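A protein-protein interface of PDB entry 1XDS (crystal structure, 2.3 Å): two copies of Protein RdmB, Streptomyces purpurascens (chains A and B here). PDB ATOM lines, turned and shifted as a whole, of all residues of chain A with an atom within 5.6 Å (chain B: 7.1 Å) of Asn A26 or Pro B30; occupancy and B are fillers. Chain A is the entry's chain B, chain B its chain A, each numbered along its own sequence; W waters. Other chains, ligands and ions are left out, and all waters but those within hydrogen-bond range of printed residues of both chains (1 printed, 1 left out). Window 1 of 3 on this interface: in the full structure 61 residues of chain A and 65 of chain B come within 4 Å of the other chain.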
ATOM      1  N   LEU A  20       6.320   4.014 -13.968  1.00  0.00           N
ATOM      2  CA  LEU A  20       6.222   5.453 -14.193  1.00  0.00           C
ATOM      3  C   LEU A  20       7.263   6.184 -13.334  1.00  0.00           C
ATOM      4  O   LEU A  20       8.064   6.957 -13.844  1.00  0.00           O
ATOM      5  CB  LEU A  20       4.809   5.967 -13.886  1.00  0.00           C
ATOM      6  CG  LEU A  20       4.586   7.464 -14.150  1.00  0.00           C
ATOM      7  CD1 LEU A  20       4.976   7.830 -15.595  1.00  0.00           C
ATOM      8  CD2 LEU A  20       3.170   7.888 -13.885  1.00  0.00           C
ATOM      9  N   LEU A  21       7.291   5.888 -12.040  1.00  0.00           N
ATOM     10  CA  LEU A  21       8.148   6.611 -11.106  1.00  0.00           C
ATOM     11  C   LEU A  21       9.652   6.333 -11.296  1.00  0.00           C
ATOM     12  O   LEU A  21      10.470   7.235 -11.103  1.00  0.00           O
ATOM     13  CB  LEU A  21       7.729   6.280  -9.671  1.00  0.00           C
ATOM     14  CG  LEU A  21       6.334   6.775  -9.265  1.00  0.00           C
ATOM     15  CD1 LEU A  21       5.836   6.130  -7.989  1.00  0.00           C
ATOM     16  CD2 LEU A  21       6.340   8.305  -9.129  1.00  0.00           C
ATOM     17  N   LYS A  22      10.003   5.102 -11.681  1.00  0.00           N
ATOM     18  CA  LYS A  22      11.398   4.645 -11.705  1.00  0.00           C
ATOM     19  C   LYS A  22      12.037   4.656 -13.084  1.00  0.00           C
ATOM     20  O   LYS A  22      13.259   4.618 -13.217  1.00  0.00           O
ATOM     21  CB  LYS A  22      11.504   3.201 -11.181  1.00  0.00           C
ATOM     22  CG  LYS A  22      11.213   3.031  -9.698  1.00  0.00           C
ATOM     23  CD  LYS A  22      11.566   1.635  -9.238  1.00  0.00           C
ATOM     24  CE  LYS A  22      11.407   1.502  -7.721  1.00  0.00           C
ATOM     25  NZ  LYS A  22      11.656   0.116  -7.242  1.00  0.00           N
ATOM     26  N   ASN A  23      11.216   4.701 -14.112  1.00  0.00           N
ATOM     27  CA  ASN A  23      11.692   4.564 -15.470  1.00  0.00           C
ATOM     28  C   ASN A  23      11.128   5.677 -16.366  1.00  0.00           C
ATOM     29  O   ASN A  23      11.830   6.620 -16.681  1.00  0.00           O
ATOM     30  CB  ASN A  23      11.322   3.152 -15.978  1.00  0.00           C
ATOM     31  CG  ASN A  23      11.675   2.926 -17.434  1.00  0.00           C
ATOM     32  OD1 ASN A  23      11.532   1.818 -17.941  1.00  0.00           O
ATOM     33  ND2 ASN A  23      12.128   3.965 -18.113  1.00  0.00           N
ATOM     34  N   LEU A  24       9.859   5.579 -16.746  1.00  0.00           N
ATOM     35  CA  LEU A  24       9.300   6.414 -17.807  1.00  0.00           C
ATOM     36  C   LEU A  24       9.201   7.903 -17.452  1.00  0.00           C
ATOM     37  O   LEU A  24       9.393   8.753 -18.305  1.00  0.00           O
ATOM     38  CB  LEU A  24       7.915   5.895 -18.226  1.00  0.00           C
ATOM     39  CG  LEU A  24       7.804   4.430 -18.681  1.00  0.00           C
ATOM     40  CD1 LEU A  24       6.340   4.108 -19.066  1.00  0.00           C
ATOM     41  CD2 LEU A  24       8.726   4.161 -19.832  1.00  0.00           C
ATOM     42  N   GLY A  25       8.909   8.201 -16.193  1.00  0.00           N
ATOM     43  CA  GLY A  25       8.832   9.565 -15.719  1.00  0.00           C
ATOM     44  C   GLY A  25      10.058  10.093 -14.997  1.00  0.00           C
ATOM     45  O   GLY A  25      10.053  11.232 -14.538  1.00  0.00           O
ATOM     46  N   ASN A  26      11.104   9.279 -14.927  1.00  0.00           N
ATOM     47  CA  ASN A  26      12.263   9.539 -14.074  1.00  0.00           C
ATOM     48  C   ASN A  26      13.344  10.319 -14.836  1.00  0.00           C
ATOM     49  O   ASN A  26      13.985   9.789 -15.744  1.00  0.00           O
ATOM     50  CB  ASN A  26      12.803   8.180 -13.561  1.00  0.00           C
ATOM     51  CG  ASN A  26      14.061   8.299 -12.689  1.00  0.00           C
ATOM     52  OD1 ASN A  26      14.598   7.283 -12.237  1.00  0.00           O
ATOM     53  ND2 ASN A  26      14.509   9.514 -12.424  1.00  0.00           N
ATOM     54  N   LEU A  27      13.546  11.575 -14.438  1.00  0.00           N
ATOM     55  CA  LEU A  27      14.547  12.475 -15.047  1.00  0.00           C
ATOM     56  C   LEU A  27      15.827  12.574 -14.198  1.00  0.00           C
ATOM     57  O   LEU A  27      16.870  13.055 -14.663  1.00  0.00           O
ATOM     58  CB  LEU A  27      13.922  13.866 -15.191  1.00  0.00           C
ATOM     59  CG  LEU A  27      14.447  14.864 -16.230  1.00  0.00           C
ATOM     60  CD1 LEU A  27      13.880  14.615 -17.632  1.00  0.00           C
ATOM     61  CD2 LEU A  27      14.103  16.280 -15.784  1.00  0.00           C
ATOM     62  N   VAL A  28      15.733  12.138 -12.948  1.00  0.00           N
ATOM     63  CA  VAL A  28      16.848  12.212 -12.002  1.00  0.00           C
ATOM     64  C   VAL A  28      17.936  11.216 -12.350  1.00  0.00           C
ATOM     65  O   VAL A  28      19.118  11.559 -12.338  1.00  0.00           O
ATOM     66  CB  VAL A  28      16.371  11.924 -10.559  1.00  0.00           C
ATOM     67  CG1 VAL A  28      17.551  11.864  -9.600  1.00  0.00           C
ATOM     68  CG2 VAL A  28      15.366  12.975 -10.130  1.00  0.00           C
ATOM     69  N   THR A  29      17.524   9.983 -12.643  1.00  0.00           N
ATOM     70  CA  THR A  29      18.448   8.901 -12.910  1.00  0.00           C
ATOM     71  C   THR A  29      19.257   9.122 -14.182  1.00  0.00           C
ATOM     72  O   THR A  29      20.480   8.991 -14.141  1.00  0.00           O
ATOM     73  CB  THR A  29      17.724   7.514 -12.921  1.00  0.00           C
ATOM     74  OG1 THR A  29      17.220   7.220 -11.608  1.00  0.00           O
ATOM     75  CG2 THR A  29      18.707   6.372 -13.199  1.00  0.00           C
ATOM     76  N   PRO A  30      18.611   9.407 -15.314  1.00  0.00           N
ATOM     77  CA  PRO A  30      19.348   9.838 -16.513  1.00  0.00           C
ATOM     78  C   PRO A  30      20.346  10.977 -16.270  1.00  0.00           C
ATOM     79  O   PRO A  30      21.430  10.960 -16.868  1.00  0.00           O
ATOM     80  CB  PRO A  30      18.244  10.276 -17.463  1.00  0.00           C
ATOM     81  CG  PRO A  30      16.984  10.241 -16.660  1.00  0.00           C
ATOM     82  CD  PRO A  30      17.178   9.249 -15.606  1.00  0.00           C
ATOM     83  N   HIS A  72      22.477   6.678  -4.855  1.00  0.00           N
ATOM     84  CA  HIS A  72      21.506   6.541  -5.923  1.00  0.00           C
ATOM     85  C   HIS A  72      22.012   5.625  -7.031  1.00  0.00           C
ATOM     86  O   HIS A  72      21.294   4.743  -7.473  1.00  0.00           O
ATOM     87  CB  HIS A  72      21.071   7.903  -6.479  1.00  0.00           C
ATOM     88  CG  HIS A  72      19.888   7.802  -7.388  1.00  0.00           C
ATOM     89  ND1 HIS A  72      19.989   7.951  -8.753  1.00  0.00           N
ATOM     90  CD2 HIS A  72      18.595   7.503  -7.134  1.00  0.00           C
ATOM     91  CE1 HIS A  72      18.798   7.784  -9.292  1.00  0.00           C
ATOM     92  NE2 HIS A  72      17.937   7.505  -8.333  1.00  0.00           N
ATOM     93  N   LYS B  22      17.071   2.673 -22.731  1.00  0.00           N
ATOM     94  CA  LYS B  22      15.621   2.869 -22.646  1.00  0.00           C
ATOM     95  C   LYS B  22      15.132   3.400 -21.309  1.00  0.00           C
ATOM     96  O   LYS B  22      14.034   3.956 -21.232  1.00  0.00           O
ATOM     97  CB  LYS B  22      14.905   1.552 -22.923  1.00  0.00           C
ATOM     98  CG  LYS B  22      15.142   1.058 -24.322  1.00  0.00           C
ATOM     99  CD  LYS B  22      14.216  -0.074 -24.709  1.00  0.00           C
ATOM    100  CE  LYS B  22      14.500  -0.498 -26.144  1.00  0.00           C
ATOM    101  NZ  LYS B  22      13.898  -1.800 -26.479  1.00  0.00           N
ATOM    102  N   ASN B  23      15.937   3.229 -20.264  1.00  0.00           N
ATOM    103  CA  ASN B  23      15.517   3.503 -18.899  1.00  0.00           C
ATOM    104  C   ASN B  23      16.512   4.450 -18.234  1.00  0.00           C
ATOM    105  O   ASN B  23      16.305   5.666 -18.231  1.00  0.00           O
ATOM    106  CB  ASN B  23      15.344   2.168 -18.129  1.00  0.00           C
ATOM    107  CG  ASN B  23      15.005   2.349 -16.626  1.00  0.00           C
ATOM    108  OD1 ASN B  23      14.540   1.411 -15.979  1.00  0.00           O
ATOM    109  ND2 ASN B  23      15.237   3.526 -16.088  1.00  0.00           N
ATOM    110  N   LEU B  24      17.613   3.897 -17.736  1.00  0.00           N
ATOM    111  CA  LEU B  24      18.524   4.615 -16.836  1.00  0.00           C
ATOM    112  C   LEU B  24      19.226   5.836 -17.442  1.00  0.00           C
ATOM    113  O   LEU B  24      19.568   6.773 -16.720  1.00  0.00           O
ATOM    114  CB  LEU B  24      19.607   3.658 -16.312  1.00  0.00           C
ATOM    115  CG  LEU B  24      19.157   2.404 -15.559  1.00  0.00           C
ATOM    116  CD1 LEU B  24      20.398   1.607 -15.137  1.00  0.00           C
ATOM    117  CD2 LEU B  24      18.297   2.711 -14.345  1.00  0.00           C
ATOM    118  N   ASN B  26      17.978   7.355 -20.323  1.00  0.00           N
ATOM    119  CA  ASN B  26      16.951   7.961 -21.164  1.00  0.00           C
ATOM    120  C   ASN B  26      16.383   9.228 -20.537  1.00  0.00           C
ATOM    121  O   ASN B  26      15.538   9.163 -19.630  1.00  0.00           O
ATOM    122  CB  ASN B  26      15.819   6.928 -21.372  1.00  0.00           C
ATOM    123  CG  ASN B  26      14.795   7.346 -22.420  1.00  0.00           C
ATOM    124  OD1 ASN B  26      13.905   6.558 -22.785  1.00  0.00           O
ATOM    125  ND2 ASN B  26      14.910   8.557 -22.909  1.00  0.00           N
ATOM    126  N   LEU B  27      16.843  10.375 -21.041  1.00  0.00           N
ATOM    127  CA  LEU B  27      16.335  11.687 -20.661  1.00  0.00           C
ATOM    128  C   LEU B  27      15.154  12.161 -21.514  1.00  0.00           C
ATOM    129  O   LEU B  27      14.480  13.112 -21.145  1.00  0.00           O
ATOM    130  CB  LEU B  27      17.467  12.708 -20.789  1.00  0.00           C
ATOM    131  CG  LEU B  27      17.428  14.011 -19.985  1.00  0.00           C
ATOM    132  CD1 LEU B  27      17.603  13.748 -18.486  1.00  0.00           C
ATOM    133  CD2 LEU B  27      18.519  14.962 -20.485  1.00  0.00           C
ATOM    134  N   VAL B  28      14.931  11.528 -22.666  1.00  0.00           N
ATOM    135  CA  VAL B  28      13.879  11.942 -23.602  1.00  0.00           C
ATOM    136  C   VAL B  28      12.480  11.566 -23.129  1.00  0.00           C
ATOM    137  O   VAL B  28      11.562  12.391 -23.118  1.00  0.00           O
ATOM    138  CB  VAL B  28      14.081  11.303 -25.006  1.00  0.00           C
ATOM    139  CG1 VAL B  28      12.946  11.722 -25.952  1.00  0.00           C
ATOM    140  CG2 VAL B  28      15.427  11.706 -25.574  1.00  0.00           C
ATOM    141  N   THR B  29      12.327  10.297 -22.782  1.00  0.00           N
ATOM    142  CA  THR B  29      11.048   9.766 -22.347  1.00  0.00           C
ATOM    143  C   THR B  29      10.451  10.502 -21.136  1.00  0.00           C
ATOM    144  O   THR B  29       9.272  10.810 -21.135  1.00  0.00           O
ATOM    145  CB  THR B  29      11.181   8.254 -22.060  1.00  0.00           C
ATOM    146  OG1 THR B  29      11.538   7.564 -23.260  1.00  0.00           O
ATOM    147  CG2 THR B  29       9.842   7.658 -21.682  1.00  0.00           C
ATOM    148  N   PRO B  30      11.215  10.738 -20.079  1.00  0.00           N
ATOM    149  CA  PRO B  30      10.691  11.527 -18.958  1.00  0.00           C
ATOM    150  C   PRO B  30      10.252  12.953 -19.328  1.00  0.00           C
ATOM    151  O   PRO B  30       9.307  13.499 -18.743  1.00  0.00           O
ATOM    152  CB  PRO B  30      11.838  11.502 -17.934  1.00  0.00           C
ATOM    153  CG  PRO B  30      12.989  10.972 -18.625  1.00  0.00           C
ATOM    154  CD  PRO B  30      12.539  10.174 -19.781  1.00  0.00           C
ATOM    155  N   MET B  31      10.916  13.563 -20.293  1.00  0.00           N
ATOM    156  CA  MET B  31      10.465  14.867 -20.735  1.00  0.00           C
ATOM    157  C   MET B  31       9.199  14.683 -21.553  1.00  0.00           C
ATOM    158  O   MET B  31       8.291  15.528 -21.467  1.00  0.00           O
ATOM    159  CB  MET B  31      11.553  15.632 -21.480  1.00  0.00           C
ATOM    160  CG  MET B  31      12.632  16.226 -20.544  1.00  0.00           C
ATOM    161  SD  MET B  31      12.019  17.239 -19.202  1.00  0.00           S
ATOM    162  CE  MET B  31      10.831  18.120 -19.999  1.00  0.00           C
ATOM    163  N   ALA B  32       9.099  13.559 -22.280  1.00  0.00           N
ATOM    164  CA  ALA B  32       7.877  13.262 -23.044  1.00  0.00           C
ATOM    165  C   ALA B  32       6.679  13.030 -22.132  1.00  0.00           C
ATOM    166  O   ALA B  32       5.535  13.441 -22.465  1.00  0.00           O
ATOM    167  CB  ALA B  32       8.061  12.078 -23.949  1.00  0.00           C
ATOM    168  N   LEU B  33       6.922  12.402 -20.981  1.00  0.00           N
ATOM    169  CA  LEU B  33       5.868  12.200 -19.999  1.00  0.00           C
ATOM    170  C   LEU B  33       5.401  13.538 -19.428  1.00  0.00           C
ATOM    171  O   LEU B  33       4.206  13.751 -19.232  1.00  0.00           O
ATOM    172  CB  LEU B  33       6.334  11.262 -18.862  1.00  0.00           C
ATOM    173  CG  LEU B  33       5.943   9.782 -19.019  1.00  0.00           C
ATOM    174  CD1 LEU B  33       4.418   9.629 -18.934  1.00  0.00           C
ATOM    175  CD2 LEU B  33       6.448   9.202 -20.356  1.00  0.00           C
ATOM    176  N   ARG B  34       6.339  14.433 -19.143  1.00  0.00           N
ATOM    177  CA  ARG B  34       6.007  15.721 -18.543  1.00  0.00           C
ATOM    178  C   ARG B  34       5.254  16.570 -19.528  1.00  0.00           C
ATOM    179  O   ARG B  34       4.268  17.187 -19.164  1.00  0.00           O
ATOM    180  CB  ARG B  34       7.266  16.461 -18.069  1.00  0.00           C
ATOM    181  CG  ARG B  34       7.829  15.851 -16.821  1.00  0.00           C
ATOM    182  CD  ARG B  34       9.188  16.338 -16.428  1.00  0.00           C
ATOM    183  NE  ARG B  34       9.527  15.859 -15.089  1.00  0.00           N
ATOM    184  CZ  ARG B  34       9.969  14.632 -14.820  1.00  0.00           C
ATOM    185  NH1 ARG B  34      10.120  13.728 -15.786  1.00  0.00           N
ATOM    186  NH2 ARG B  34      10.241  14.294 -13.568  1.00  0.00           N
ATOM    187  N   VAL B  35       5.700  16.612 -20.779  1.00  0.00           N
ATOM    188  CA  VAL B  35       4.913  17.285 -21.807  1.00  0.00           C
ATOM    189  C   VAL B  35       3.488  16.716 -21.912  1.00  0.00           C
ATOM    190  O   VAL B  35       2.544  17.487 -22.026  1.00  0.00           O
ATOM    191  CB  VAL B  35       5.627  17.327 -23.192  1.00  0.00           C
ATOM    192  CG1 VAL B  35       4.703  17.860 -24.265  1.00  0.00           C
ATOM    193  CG2 VAL B  35       6.848  18.225 -23.117  1.00  0.00           C
ATOM    194  N   ALA B  36       3.314  15.396 -21.841  1.00  0.00           N
ATOM    195  CA  ALA B  36       1.977  14.800 -21.978  1.00  0.00           C
ATOM    196  C   ALA B  36       1.113  15.144 -20.784  1.00  0.00           C
ATOM    197  O   ALA B  36      -0.077  15.394 -20.915  1.00  0.00           O
ATOM    198  CB  ALA B  36       2.074  13.248 -22.118  1.00  0.00           C
ATOM    199  N   HIS B  72       6.040   8.319 -29.872  1.00  0.00           N
ATOM    200  CA  HIS B  72       6.940   7.988 -28.767  1.00  0.00           C
ATOM    201  C   HIS B  72       6.189   7.486 -27.547  1.00  0.00           C
ATOM    202  O   HIS B  72       6.641   6.542 -26.887  1.00  0.00           O
ATOM    203  CB  HIS B  72       7.808   9.170 -28.365  1.00  0.00           C
ATOM    204  CG  HIS B  72       8.961   8.782 -27.495  1.00  0.00           C
ATOM    205  ND1 HIS B  72       8.888   8.798 -26.120  1.00  0.00           N
ATOM    206  CD2 HIS B  72      10.201   8.342 -27.801  1.00  0.00           C
ATOM    207  CE1 HIS B  72      10.037   8.381 -25.618  1.00  0.00           C
ATOM    208  NE2 HIS B  72      10.850   8.096 -26.618  1.00  0.00           N
ATOM    209  N   LEU B 110       3.924  15.689 -12.567  1.00  0.00           N
ATOM    210  CA  LEU B 110       4.727  15.779 -13.774  1.00  0.00           C
ATOM    211  C   LEU B 110       4.486  17.083 -14.531  1.00  0.00           C
ATOM    212  O   LEU B 110       5.272  17.430 -15.410  1.00  0.00           O
ATOM    213  CB  LEU B 110       4.414  14.593 -14.674  1.00  0.00           C
ATOM    214  CG  LEU B 110       4.892  13.239 -14.130  1.00  0.00           C
ATOM    215  CD1 LEU B 110       4.130  12.090 -14.819  1.00  0.00           C
ATOM    216  CD2 LEU B 110       6.382  13.078 -14.323  1.00  0.00           C
ATOM    217  N   LEU B 112       4.505  20.560 -16.132  1.00  0.00           N
ATOM    218  CA  LEU B 112       5.615  21.531 -16.258  1.00  0.00           C
ATOM    219  C   LEU B 112       5.205  22.933 -15.800  1.00  0.00           C
ATOM    220  O   LEU B 112       6.048  23.759 -15.530  1.00  0.00           O
ATOM    221  CB  LEU B 112       6.169  21.584 -17.697  1.00  0.00           C
ATOM    222  CG  LEU B 112       6.974  20.374 -18.215  1.00  0.00           C
ATOM    223  CD1 LEU B 112       7.068  20.333 -19.753  1.00  0.00           C
ATOM    224  CD2 LEU B 112       8.372  20.367 -17.607  1.00  0.00           C
ATOM    225  N   SER B 117       7.771  19.553 -11.193  1.00  0.00           N
ATOM    226  CA  SER B 117       8.341  19.290 -12.523  1.00  0.00           C
ATOM    227  C   SER B 117       9.198  20.482 -12.992  1.00  0.00           C
ATOM    228  O   SER B 117      10.269  20.306 -13.558  1.00  0.00           O
ATOM    229  CB  SER B 117       7.220  19.041 -13.508  1.00  0.00           C
ATOM    230  OG  SER B 117       7.695  18.373 -14.635  1.00  0.00           O
ATOM    231  N   PHE B 299      15.192   3.381  -3.609  1.00  0.00           N
ATOM    232  CA  PHE B 299      14.998   4.223  -4.796  1.00  0.00           C
ATOM    233  C   PHE B 299      14.335   5.541  -4.425  1.00  0.00           C
ATOM    234  O   PHE B 299      14.800   6.598  -4.812  1.00  0.00           O
ATOM    235  CB  PHE B 299      14.176   3.541  -5.907  1.00  0.00           C
ATOM    236  CG  PHE B 299      13.967   4.422  -7.106  1.00  0.00           C
ATOM    237  CD1 PHE B 299      14.882   4.431  -8.138  1.00  0.00           C
ATOM    238  CD2 PHE B 299      12.883   5.295  -7.166  1.00  0.00           C
ATOM    239  CE1 PHE B 299      14.710   5.268  -9.230  1.00  0.00           C
ATOM    240  CE2 PHE B 299      12.699   6.128  -8.249  1.00  0.00           C
ATOM    241  CZ  PHE B 299      13.613   6.123  -9.282  1.00  0.00           C
ATOM    242  N   LEU B 303      16.091   9.263  -4.476  1.00  0.00           N
ATOM    243  CA  LEU B 303      15.465  10.191  -5.422  1.00  0.00           C
ATOM    244  C   LEU B 303      15.109  11.474  -4.718  1.00  0.00           C
ATOM    245  O   LEU B 303      15.517  12.551  -5.118  1.00  0.00           O
ATOM    246  CB  LEU B 303      14.192   9.577  -6.043  1.00  0.00           C
ATOM    247  CG  LEU B 303      13.373  10.415  -7.044  1.00  0.00           C
ATOM    248  CD1 LEU B 303      14.105  10.497  -8.354  1.00  0.00           C
ATOM    249  CD2 LEU B 303      11.988   9.826  -7.308  1.00  0.00           C
ATOM    250  N   ARG B 307      16.667  15.284  -5.023  1.00  0.00           N
ATOM    251  CA  ARG B 307      15.788  16.418  -5.214  1.00  0.00           C
ATOM    252  C   ARG B 307      15.960  17.466  -4.143  1.00  0.00           C
ATOM    253  O   ARG B 307      15.912  18.639  -4.461  1.00  0.00           O
ATOM    254  CB  ARG B 307      14.312  15.999  -5.198  1.00  0.00           C
ATOM    255  CG  ARG B 307      13.776  15.380  -6.462  1.00  0.00           C
ATOM    256  CD  ARG B 307      12.245  15.348  -6.518  1.00  0.00           C
ATOM    257  NE  ARG B 307      11.805  15.005  -7.858  1.00  0.00           N
ATOM    258  CZ  ARG B 307      10.720  14.298  -8.175  1.00  0.00           C
ATOM    259  NH1 ARG B 307       9.865  13.865  -7.256  1.00  0.00           N
ATOM    260  NH2 ARG B 307      10.475  14.050  -9.449  1.00  0.00           N
HETATM  261  O   HOH W   1      15.372   5.881 -15.136  1.00  0.00           O
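Phe B299 touches Leu A21. Lys B22 touches Asn A23. Asn B23 touches Asn A23 (CG to CG, 3.5 Å). Thr B29 touches Leu A24 (C to O, 3.5 Å). Leu A24 touches Leu B33. OD1 of Asn A26 touches CZ of Phe B299, 3.3 Å away. NH1 of Arg B34 touches CB of Leu A27, at 3.9 Å. Val A28 touches Leu B303. Thr A29 touches Phe B299 (OG1 to CE1, 3.97 Å). CG of Pro A30 touches O of Asn B26 (3.5 Å).
Lys A22 touches Asn B23, and with the chains exchanged Asn A23 touches Lys B22. Leu A24 touches Pro B30, and with the chains exchanged Pro A30 touches Leu B24. Leu A27 touches its own counterpart, Leu B27. Leu A27 touches Pro B30, and with the chains exchanged Pro A30 touches Leu B27.
Of the printed residues of chain B, Leu A20 touches Leu B33. Gly A25 touches just these residues of chain B: Pro B30 and Arg B34. Printed residues of chain B within 4 Å of Asn A26: Pro B30 and Phe B299. Of the printed residues of chain A, Asn B23 touches Lys A22 (3.7 Å) and Asn A23 (3.5 Å). Val B28 touches none of the printed residues of chain A. Pro B30 touches four residues of chain A. The nearest printed residue of chain B that does not touch Asn A26 is Leu B303 (4.2 Å). The nearest residue of chain A that does not touch Pro B30 is Pro A30 (4.5 Å). The nearest printed residue of chain A that does not touch Leu B27 is Asn A26 (5.8 Å).
Of the 12 printed residues of chain A, 11 touch a printed residue of chain B. Printed residues of chain A that touch a printed residue of chain B: Leu A20, Leu A21, Lys A22, Asn A23, Leu A24, Gly A25, Asn A26, Leu A27, Val A28, Thr A29 and Pro A30. Printed residues of chain B that touch a printed residue of chain A: Lys B22, Asn B23, Leu B24, Asn B26, Leu B27, Thr B29, Pro B30, Met B31, Leu B33, Arg B34, Phe B299 and Leu B303. Among the printed residues, 23 pairs touch across the chains.
The guanidinium group (NH1) of Arg B34 lies within hydrogen-bond range of the backbone carbonyl oxygen (O) of Gly A25, at 2.8 Å. The backbone carbonyl oxygen (O) of Leu A24 lies close to the backbone nitrogen (N) of Pro B30, 3.2 Å away. The backbone nitrogen (N) of Pro A30 lies close to the backbone carbonyl oxygen (O) of Leu B24 (3.1 Å).
Water W1 lies within hydrogen-bond range of the side-chain amide nitrogen of Asn B23, the backbone carbonyl oxygen of Lys A22 and the side-chain amide oxygen of Asn A26.
The backbone carbonyl oxygen of Lys B22 lies close to the side-chain amide oxygen of Asn B26 (3.0 Å). The backbone NH (N) of Val B28 sits close to the side-chain amide nitrogen (ND2) of Asn B26, at 3.0 Å. The side-chain hydroxyl of Thr B29 sits close to a ring nitrogen (NE2) of His B72. The guanidinium group of Arg B34 sits at hydrogen-bond distance from the backbone carbonyl oxygen of Pro B30, at 3.1 Å. The backbone carbonyl oxygen (O) of Leu A20 is in hydrogen-bond range of the backbone NH (N) of Gly A25, 2.8 Å away. ND2 of Asn A26 lies close to N of Val A28.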
